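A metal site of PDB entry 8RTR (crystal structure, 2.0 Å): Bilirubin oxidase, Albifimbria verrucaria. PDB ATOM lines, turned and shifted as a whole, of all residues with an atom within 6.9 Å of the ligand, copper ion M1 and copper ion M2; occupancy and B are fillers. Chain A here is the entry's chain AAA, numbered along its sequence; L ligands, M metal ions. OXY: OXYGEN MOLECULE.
NE2 of His 96 lies close to ND1 of His 401.
The backbone NH (N) of His 96 lies within hydrogen-bond range of the backbone carbonyl oxygen (O) of Trp 132, at 2.8 Å.
NE2 of His 96 lies within hydrogen-bond range of NH2 of Arg 276 (3.2 Å).
The backbone NH (N) of His 403 sits at hydrogen-bond distance from the backbone carbonyl oxygen (O) of Met 454, at 3.1 Å.
The side-chain carboxylate (OD2) of Asp 105 sits at hydrogen-bond distance from a ring nitrogen (ND1) of His 403, at 2.7 Å.
The backbone carbonyl oxygen (O) of His 456 is in hydrogen-bond range of the backbone NH (N) of His 401 (2.8 Å).
ND1 of His 456 lies close to OE1 of Glu 463 (3.2 Å).
A ring nitrogen (ND1) of His 94 sits at hydrogen-bond distance from the backbone carbonyl oxygen (O) of Asp 105 (2.6 Å).
His 401 touches copper ion M2.
Four residues have an atom within 4 Å of copper ion M2: His 136, His 401, His 403 and His 456.
Copper ion M1 is bound by a ring nitrogen (ND1) of His 96 (2.0 Å), a ring nitrogen (NE2) of His 134 (2.1 Å), a ring nitrogen (NE2) of His 458 (2.3 Å) and an oxygen (O2) of the ligand (2.5 Å).
Copper ion M1 has four donor atoms within binding distance.
O1 of the ligand sits close to NE2 of His 94 (3.5 Å).
An oxygen (O1) of the ligand lies close to a ring nitrogen (NE2) of His 401 (3.4 Å).
Hydrophobic or aromatic side chains within 4 Å of the ligand: His 94, His 96, His 134, His 136, His 401, His 403, His 456 and His 458.
His 94 touches copper ion M1.
CZ2 of Trp 132 touches copper ion M1, at 3.6 Å.
Within 4 Å of copper ion M1: His 94, His 96, Trp 132, His 134 and His 458.
The nearest printed residue that does not touch copper ion M1 is Ala 274 (4.3 Å).
Copper ion M2 is bound by a ring nitrogen (NE2) of His 136 (1.9 Å), a ring nitrogen (NE2) of His 403 (2.0 Å), a ring nitrogen (NE2) of His 456 (2.1 Å) and an oxygen (O1) of the ligand (2.4 Å).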
ATOM      1  N   HIS A  94      -0.361  11.099 -25.983  1.00  0.00           N
ATOM      2  CA  HIS A  94       0.105  11.616 -24.677  1.00  0.00           C
ATOM      3  C   HIS A  94      -0.912  12.579 -24.075  1.00  0.00           C
ATOM      4  O   HIS A  94      -1.263  13.555 -24.761  1.00  0.00           O
ATOM      5  CB  HIS A  94       1.441  12.303 -24.869  1.00  0.00           C
ATOM      6  CG  HIS A  94       1.920  13.011 -23.656  1.00  0.00           C
ATOM      7  ND1 HIS A  94       2.054  12.368 -22.458  1.00  0.00           N
ATOM      8  CD2 HIS A  94       2.328  14.277 -23.470  1.00  0.00           C
ATOM      9  CE1 HIS A  94       2.504  13.213 -21.568  1.00  0.00           C
ATOM     10  NE2 HIS A  94       2.695  14.385 -22.177  1.00  0.00           N
ATOM     11  N   LEU A  95      -1.327  12.320 -22.834  1.00  0.00           N
ATOM     12  CA  LEU A  95      -2.054  13.277 -21.963  1.00  0.00           C
ATOM     13  C   LEU A  95      -1.020  14.116 -21.194  1.00  0.00           C
ATOM     14  O   LEU A  95      -0.458  13.643 -20.177  1.00  0.00           O
ATOM     15  CB  LEU A  95      -2.978  12.524 -20.980  1.00  0.00           C
ATOM     16  CG  LEU A  95      -3.877  13.406 -20.118  1.00  0.00           C
ATOM     17  CD1 LEU A  95      -4.729  14.315 -20.962  1.00  0.00           C
ATOM     18  CD2 LEU A  95      -4.785  12.561 -19.227  1.00  0.00           C
ATOM     19  N   HIS A  96      -0.751  15.300 -21.716  1.00  0.00           N
ATOM     20  CA  HIS A  96       0.235  16.261 -21.196  1.00  0.00           C
ATOM     21  C   HIS A  96      -0.367  16.918 -19.931  1.00  0.00           C
ATOM     22  O   HIS A  96      -1.405  17.594 -20.009  1.00  0.00           O
ATOM     23  CB  HIS A  96       0.606  17.209 -22.359  1.00  0.00           C
ATOM     24  CG  HIS A  96       1.740  18.136 -22.065  1.00  0.00           C
ATOM     25  ND1 HIS A  96       2.694  18.447 -23.000  1.00  0.00           N
ATOM     26  CD2 HIS A  96       2.080  18.797 -20.929  1.00  0.00           C
ATOM     27  CE1 HIS A  96       3.564  19.291 -22.467  1.00  0.00           C
ATOM     28  NE2 HIS A  96       3.229  19.514 -21.189  1.00  0.00           N
ATOM     29  N   GLY A  97       0.262  16.691 -18.784  1.00  0.00           N
ATOM     30  CA  GLY A  97      -0.179  17.234 -17.495  1.00  0.00           C
ATOM     31  C   GLY A  97      -0.605  16.127 -16.547  1.00  0.00           C
ATOM     32  O   GLY A  97      -0.961  16.493 -15.428  1.00  0.00           O
ATOM     33  N   ASP A 105       1.371   6.769 -21.296  1.00  0.00           N
ATOM     34  CA  ASP A 105       1.916   8.145 -21.258  1.00  0.00           C
ATOM     35  C   ASP A 105       2.235   8.661 -22.656  1.00  0.00           C
ATOM     36  O   ASP A 105       2.500   9.852 -22.786  1.00  0.00           O
ATOM     37  CB  ASP A 105       3.167   8.265 -20.385  1.00  0.00           C
ATOM     38  CG  ASP A 105       3.519   9.707 -19.998  1.00  0.00           C
ATOM     39  OD1 ASP A 105       2.578  10.463 -19.569  1.00  0.00           O
ATOM     40  OD2 ASP A 105       4.724  10.059 -20.129  1.00  0.00           O
ATOM     41  N   GLY A 106       2.177   7.816 -23.674  1.00  0.00           N
ATOM     42  CA  GLY A 106       2.479   8.251 -25.047  1.00  0.00           C
ATOM     43  C   GLY A 106       3.966   8.183 -25.353  1.00  0.00           C
ATOM     44  O   GLY A 106       4.439   8.961 -26.206  1.00  0.00           O
ATOM     45  N   TRP A 132      -3.810  18.675 -21.910  1.00  0.00           N
ATOM     46  CA  TRP A 132      -4.158  18.528 -23.332  1.00  0.00           C
ATOM     47  C   TRP A 132      -3.645  17.167 -23.792  1.00  0.00           C
ATOM     48  O   TRP A 132      -2.634  16.710 -23.226  1.00  0.00           O
ATOM     49  CB  TRP A 132      -3.692  19.731 -24.165  1.00  0.00           C
ATOM     50  CG  TRP A 132      -2.207  19.935 -24.270  1.00  0.00           C
ATOM     51  CD1 TRP A 132      -1.314  20.131 -23.257  1.00  0.00           C
ATOM     52  CD2 TRP A 132      -1.463  20.086 -25.496  1.00  0.00           C
ATOM     53  NE1 TRP A 132      -0.052  20.330 -23.763  1.00  0.00           N
ATOM     54  CE2 TRP A 132      -0.113  20.327 -25.125  1.00  0.00           C
ATOM     55  CE3 TRP A 132      -1.796  20.067 -26.852  1.00  0.00           C
ATOM     56  CZ2 TRP A 132       0.885  20.541 -26.073  1.00  0.00           C
ATOM     57  CZ3 TRP A 132      -0.801  20.261 -27.789  1.00  0.00           C
ATOM     58  CH2 TRP A 132       0.522  20.472 -27.407  1.00  0.00           C
ATOM     59  N   HIS A 134      -2.509  14.835 -27.194  1.00  0.00           N
ATOM     60  CA  HIS A 134      -1.917  15.082 -28.534  1.00  0.00           C
ATOM     61  C   HIS A 134      -0.971  13.959 -28.899  1.00  0.00           C
ATOM     62  O   HIS A 134      -0.537  13.169 -28.025  1.00  0.00           O
ATOM     63  CB  HIS A 134      -1.187  16.442 -28.600  1.00  0.00           C
ATOM     64  CG  HIS A 134       0.026  16.537 -27.732  1.00  0.00           C
ATOM     65  ND1 HIS A 134       1.194  15.920 -28.045  1.00  0.00           N
ATOM     66  CD2 HIS A 134       0.267  17.200 -26.586  1.00  0.00           C
ATOM     67  CE1 HIS A 134       2.128  16.193 -27.143  1.00  0.00           C
ATOM     68  NE2 HIS A 134       1.584  16.990 -26.240  1.00  0.00           N
ATOM     69  N   ASP A 135      -0.605  13.951 -30.173  1.00  0.00           N
ATOM     70  CA  ASP A 135       0.181  12.840 -30.710  1.00  0.00           C
ATOM     71  C   ASP A 135       1.608  12.971 -30.212  1.00  0.00           C
ATOM     72  O   ASP A 135       2.077  14.144 -30.023  1.00  0.00           O
ATOM     73  CB  ASP A 135       0.099  12.781 -32.229  1.00  0.00           C
ATOM     74  CG  ASP A 135       0.666  11.469 -32.701  1.00  0.00           C
ATOM     75  OD1 ASP A 135       0.093  10.398 -32.315  1.00  0.00           O
ATOM     76  OD2 ASP A 135       1.721  11.503 -33.347  1.00  0.00           O
ATOM     77  N   HIS A 136       2.270  11.839 -30.043  1.00  0.00           N
ATOM     78  CA  HIS A 136       3.687  11.781 -29.609  1.00  0.00           C
ATOM     79  C   HIS A 136       4.461  10.735 -30.414  1.00  0.00           C
ATOM     80  O   HIS A 136       5.542  10.316 -29.966  1.00  0.00           O
ATOM     81  CB  HIS A 136       3.680  11.505 -28.113  1.00  0.00           C
ATOM     82  CG  HIS A 136       4.764  12.184 -27.354  1.00  0.00           C
ATOM     83  ND1 HIS A 136       6.082  11.995 -27.648  1.00  0.00           N
ATOM     84  CD2 HIS A 136       4.717  13.017 -26.273  1.00  0.00           C
ATOM     85  CE1 HIS A 136       6.823  12.731 -26.831  1.00  0.00           C
ATOM     86  NE2 HIS A 136       6.013  13.341 -25.953  1.00  0.00           N
ATOM     87  N   THR A 141       5.589  13.555 -34.799  1.00  0.00           N
ATOM     88  CA  THR A 141       4.737  14.284 -33.826  1.00  0.00           C
ATOM     89  C   THR A 141       4.384  15.671 -34.409  1.00  0.00           C
ATOM     90  O   THR A 141       3.245  16.083 -34.286  1.00  0.00           O
ATOM     91  CB  THR A 141       5.436  14.417 -32.467  1.00  0.00           C
ATOM     92  OG1 THR A 141       5.593  13.096 -31.987  1.00  0.00           O
ATOM     93  CG2 THR A 141       4.631  15.258 -31.495  1.00  0.00           C
ATOM     94  N   ALA A 274       3.320  24.207 -25.670  1.00  0.00           N
ATOM     95  CA  ALA A 274       2.823  23.229 -24.680  1.00  0.00           C
ATOM     96  C   ALA A 274       2.549  23.893 -23.324  1.00  0.00           C
ATOM     97  O   ALA A 274       2.013  23.225 -22.455  1.00  0.00           O
ATOM     98  CB  ALA A 274       3.773  22.066 -24.531  1.00  0.00           C
ATOM     99  N   ARG A 276       0.404  25.982 -20.747  1.00  0.00           N
ATOM    100  CA  ARG A 276      -1.002  26.419 -20.465  1.00  0.00           C
ATOM    101  C   ARG A 276      -0.935  27.530 -19.423  1.00  0.00           C
ATOM    102  O   ARG A 276      -0.268  27.351 -18.368  1.00  0.00           O
ATOM    103  CB  ARG A 276      -1.902  25.287 -19.953  1.00  0.00           C
ATOM    104  CG  ARG A 276      -2.202  24.176 -20.961  1.00  0.00           C
ATOM    105  CD  ARG A 276      -1.075  23.160 -21.042  1.00  0.00           C
ATOM    106  NE  ARG A 276      -0.965  22.333 -19.845  1.00  0.00           N
ATOM    107  CZ  ARG A 276       0.146  21.727 -19.439  1.00  0.00           C
ATOM    108  NH1 ARG A 276       0.139  21.002 -18.340  1.00  0.00           N
ATOM    109  NH2 ARG A 276       1.273  21.866 -20.119  1.00  0.00           N
ATOM    110  N   HIS A 401      10.112  20.259 -21.620  1.00  0.00           N
ATOM    111  CA  HIS A 401       9.013  19.530 -20.962  1.00  0.00           C
ATOM    112  C   HIS A 401       9.586  18.293 -20.293  1.00  0.00           C
ATOM    113  O   HIS A 401      10.413  17.627 -20.904  1.00  0.00           O
ATOM    114  CB  HIS A 401       7.949  19.187 -21.994  1.00  0.00           C
ATOM    115  CG  HIS A 401       6.848  18.377 -21.424  1.00  0.00           C
ATOM    116  ND1 HIS A 401       6.269  18.678 -20.196  1.00  0.00           N
ATOM    117  CD2 HIS A 401       6.210  17.287 -21.911  1.00  0.00           C
ATOM    118  CE1 HIS A 401       5.333  17.799 -19.953  1.00  0.00           C
ATOM    119  NE2 HIS A 401       5.296  16.916 -20.986  1.00  0.00           N
ATOM    120  N   ILE A 402       9.134  18.005 -19.084  1.00  0.00           N
ATOM    121  CA  ILE A 402       9.494  16.758 -18.386  1.00  0.00           C
ATOM    122  C   ILE A 402       8.176  16.028 -18.080  1.00  0.00           C
ATOM    123  O   ILE A 402       7.305  16.586 -17.339  1.00  0.00           O
ATOM    124  CB  ILE A 402      10.318  17.061 -17.120  1.00  0.00           C
ATOM    125  CG1 ILE A 402      11.532  17.949 -17.390  1.00  0.00           C
ATOM    126  CG2 ILE A 402      10.689  15.759 -16.435  1.00  0.00           C
ATOM    127  CD1 ILE A 402      12.221  18.458 -16.140  1.00  0.00           C
ATOM    128  N   HIS A 403       8.068  14.793 -18.561  1.00  0.00           N
ATOM    129  CA  HIS A 403       6.906  13.908 -18.304  1.00  0.00           C
ATOM    130  C   HIS A 403       6.868  13.532 -16.816  1.00  0.00           C
ATOM    131  O   HIS A 403       7.846  13.755 -16.105  1.00  0.00           O
ATOM    132  CB  HIS A 403       6.959  12.662 -19.220  1.00  0.00           C
ATOM    133  CG  HIS A 403       6.626  12.960 -20.646  1.00  0.00           C
ATOM    134  ND1 HIS A 403       5.669  12.276 -21.321  1.00  0.00           N
ATOM    135  CD2 HIS A 403       7.119  13.887 -21.507  1.00  0.00           C
ATOM    136  CE1 HIS A 403       5.602  12.722 -22.566  1.00  0.00           C
ATOM    137  NE2 HIS A 403       6.488  13.737 -22.703  1.00  0.00           N
ATOM    138  N   VAL A 431       6.345  22.613 -18.456  1.00  0.00           N
ATOM    139  CA  VAL A 431       7.112  23.171 -19.586  1.00  0.00           C
ATOM    140  C   VAL A 431       7.819  24.453 -19.105  1.00  0.00           C
ATOM    141  O   VAL A 431       7.181  25.236 -18.368  1.00  0.00           O
ATOM    142  CB  VAL A 431       6.175  23.469 -20.762  1.00  0.00           C
ATOM    143  CG1 VAL A 431       6.935  23.885 -22.022  1.00  0.00           C
ATOM    144  CG2 VAL A 431       5.295  22.263 -21.075  1.00  0.00           C
ATOM    145  N   MET A 454       9.846  10.300 -20.855  1.00  0.00           N
ATOM    146  CA  MET A 454      10.521  11.217 -21.780  1.00  0.00           C
ATOM    147  C   MET A 454      10.675  12.599 -21.134  1.00  0.00           C
ATOM    148  O   MET A 454       9.893  12.976 -20.219  1.00  0.00           O
ATOM    149  CB  MET A 454       9.727  11.334 -23.080  1.00  0.00           C
ATOM    150  CG  MET A 454       9.679  10.016 -23.839  1.00  0.00           C
ATOM    151  SD  MET A 454       8.656  10.023 -25.310  1.00  0.00           S
ATOM    152  CE  MET A 454       7.052  10.429 -24.630  1.00  0.00           C
ATOM    153  N   PHE A 455      11.671  13.330 -21.609  1.00  0.00           N
ATOM    154  CA  PHE A 455      11.799  14.801 -21.458  1.00  0.00           C
ATOM    155  C   PHE A 455      12.464  15.306 -22.735  1.00  0.00           C
ATOM    156  O   PHE A 455      13.202  14.544 -23.399  1.00  0.00           O
ATOM    157  CB  PHE A 455      12.563  15.188 -20.186  1.00  0.00           C
ATOM    158  CG  PHE A 455      14.053  14.959 -20.195  1.00  0.00           C
ATOM    159  CD1 PHE A 455      14.566  13.685 -19.995  1.00  0.00           C
ATOM    160  CD2 PHE A 455      14.948  16.011 -20.366  1.00  0.00           C
ATOM    161  CE1 PHE A 455      15.942  13.479 -19.977  1.00  0.00           C
ATOM    162  CE2 PHE A 455      16.313  15.801 -20.340  1.00  0.00           C
ATOM    163  CZ  PHE A 455      16.802  14.530 -20.135  1.00  0.00           C
ATOM    164  N   HIS A 456      12.136  16.518 -23.119  1.00  0.00           N
ATOM    165  CA  HIS A 456      12.453  16.982 -24.481  1.00  0.00           C
ATOM    166  C   HIS A 456      12.061  18.437 -24.625  1.00  0.00           C
ATOM    167  O   HIS A 456      11.230  18.931 -23.844  1.00  0.00           O
ATOM    168  CB  HIS A 456      11.705  16.127 -25.523  1.00  0.00           C
ATOM    169  CG  HIS A 456      10.228  16.127 -25.335  1.00  0.00           C
ATOM    170  ND1 HIS A 456       9.391  16.966 -26.031  1.00  0.00           N
ATOM    171  CD2 HIS A 456       9.435  15.377 -24.541  1.00  0.00           C
ATOM    172  CE1 HIS A 456       8.155  16.707 -25.680  1.00  0.00           C
ATOM    173  NE2 HIS A 456       8.162  15.751 -24.767  1.00  0.00           N
ATOM    174  N   CYS A 457      12.523  19.013 -25.727  1.00  0.00           N
ATOM    175  CA  CYS A 457      11.994  20.291 -26.236  1.00  0.00           C
ATOM    176  C   CYS A 457      10.624  20.025 -26.883  1.00  0.00           C
ATOM    177  O   CYS A 457      10.445  18.973 -27.538  1.00  0.00           O
ATOM    178  CB  CYS A 457      13.027  20.921 -27.146  1.00  0.00           C
ATOM    179  SG  CYS A 457      12.410  22.408 -27.962  1.00  0.00           S
ATOM    180  N   HIS A 458       9.690  20.955 -26.703  1.00  0.00           N
ATOM    181  CA  HIS A 458       8.309  20.905 -27.262  1.00  0.00           C
ATOM    182  C   HIS A 458       8.153  21.788 -28.498  1.00  0.00           C
ATOM    183  O   HIS A 458       7.042  21.881 -28.998  1.00  0.00           O
ATOM    184  CB  HIS A 458       7.296  21.298 -26.193  1.00  0.00           C
ATOM    185  CG  HIS A 458       6.060  20.469 -26.277  1.00  0.00           C
ATOM    186  ND1 HIS A 458       5.151  20.632 -27.295  1.00  0.00           N
ATOM    187  CD2 HIS A 458       5.606  19.460 -25.509  1.00  0.00           C
ATOM    188  CE1 HIS A 458       4.176  19.753 -27.139  1.00  0.00           C
ATOM    189  NE2 HIS A 458       4.416  19.049 -26.028  1.00  0.00           N
ATOM    190  N   LEU A 460       8.177  21.012 -31.908  1.00  0.00           N
ATOM    191  CA  LEU A 460       7.907  19.642 -32.359  1.00  0.00           C
ATOM    192  C   LEU A 460       8.878  19.288 -33.500  1.00  0.00           C
ATOM    193  O   LEU A 460       9.203  18.121 -33.667  1.00  0.00           O
ATOM    194  CB  LEU A 460       6.445  19.555 -32.765  1.00  0.00           C
ATOM    195  CG  LEU A 460       5.420  19.822 -31.649  1.00  0.00           C
ATOM    196  CD1 LEU A 460       4.023  19.565 -32.170  1.00  0.00           C
ATOM    197  CD2 LEU A 460       5.672  18.962 -30.427  1.00  0.00           C
ATOM    198  N   GLU A 463      11.955  18.306 -31.495  1.00  0.00           N
ATOM    199  CA  GLU A 463      11.575  17.033 -30.813  1.00  0.00           C
ATOM    200  C   GLU A 463      11.729  15.838 -31.777  1.00  0.00           C
ATOM    201  O   GLU A 463      12.312  14.817 -31.384  1.00  0.00           O
ATOM    202  CB  GLU A 463      10.123  17.117 -30.322  1.00  0.00           C
ATOM    203  CG  GLU A 463       9.667  15.939 -29.514  1.00  0.00           C
ATOM    204  CD  GLU A 463       8.237  16.042 -29.047  1.00  0.00           C
ATOM    205  OE1 GLU A 463       7.775  17.221 -28.772  1.00  0.00           O
ATOM    206  OE2 GLU A 463       7.590  14.956 -28.919  1.00  0.00           O
ATOM    207  N   MET A 468      15.151  14.892 -27.711  1.00  0.00           N
ATOM    208  CA  MET A 468      14.354  14.146 -26.731  1.00  0.00           C
ATOM    209  C   MET A 468      15.221  13.069 -26.119  1.00  0.00           C
ATOM    210  O   MET A 468      16.145  12.605 -26.793  1.00  0.00           O
ATOM    211  CB  MET A 468      13.147  13.524 -27.418  1.00  0.00           C
ATOM    212  CG  MET A 468      12.214  12.756 -26.498  1.00  0.00           C
ATOM    213  SD  MET A 468      10.589  12.819 -27.277  1.00  0.00           S
ATOM    214  CE  MET A 468      10.875  11.681 -28.645  1.00  0.00           C
HETATM  215  O1  OXY L   1       4.756  16.200 -24.311  1.00  0.00           O
HETATM  216  O2  OXY L   1       4.571  16.081 -25.410  1.00  0.00           O
HETATM  217 CU    CU M   1       2.876  17.840 -24.862  1.00  0.00          CU
HETATM  218 CU    CU M   2       6.440  14.541 -24.510  1.00  0.00          CU
HETATM  219 CU    CU M   3       3.963  15.667 -21.603  1.00  0.00          CU
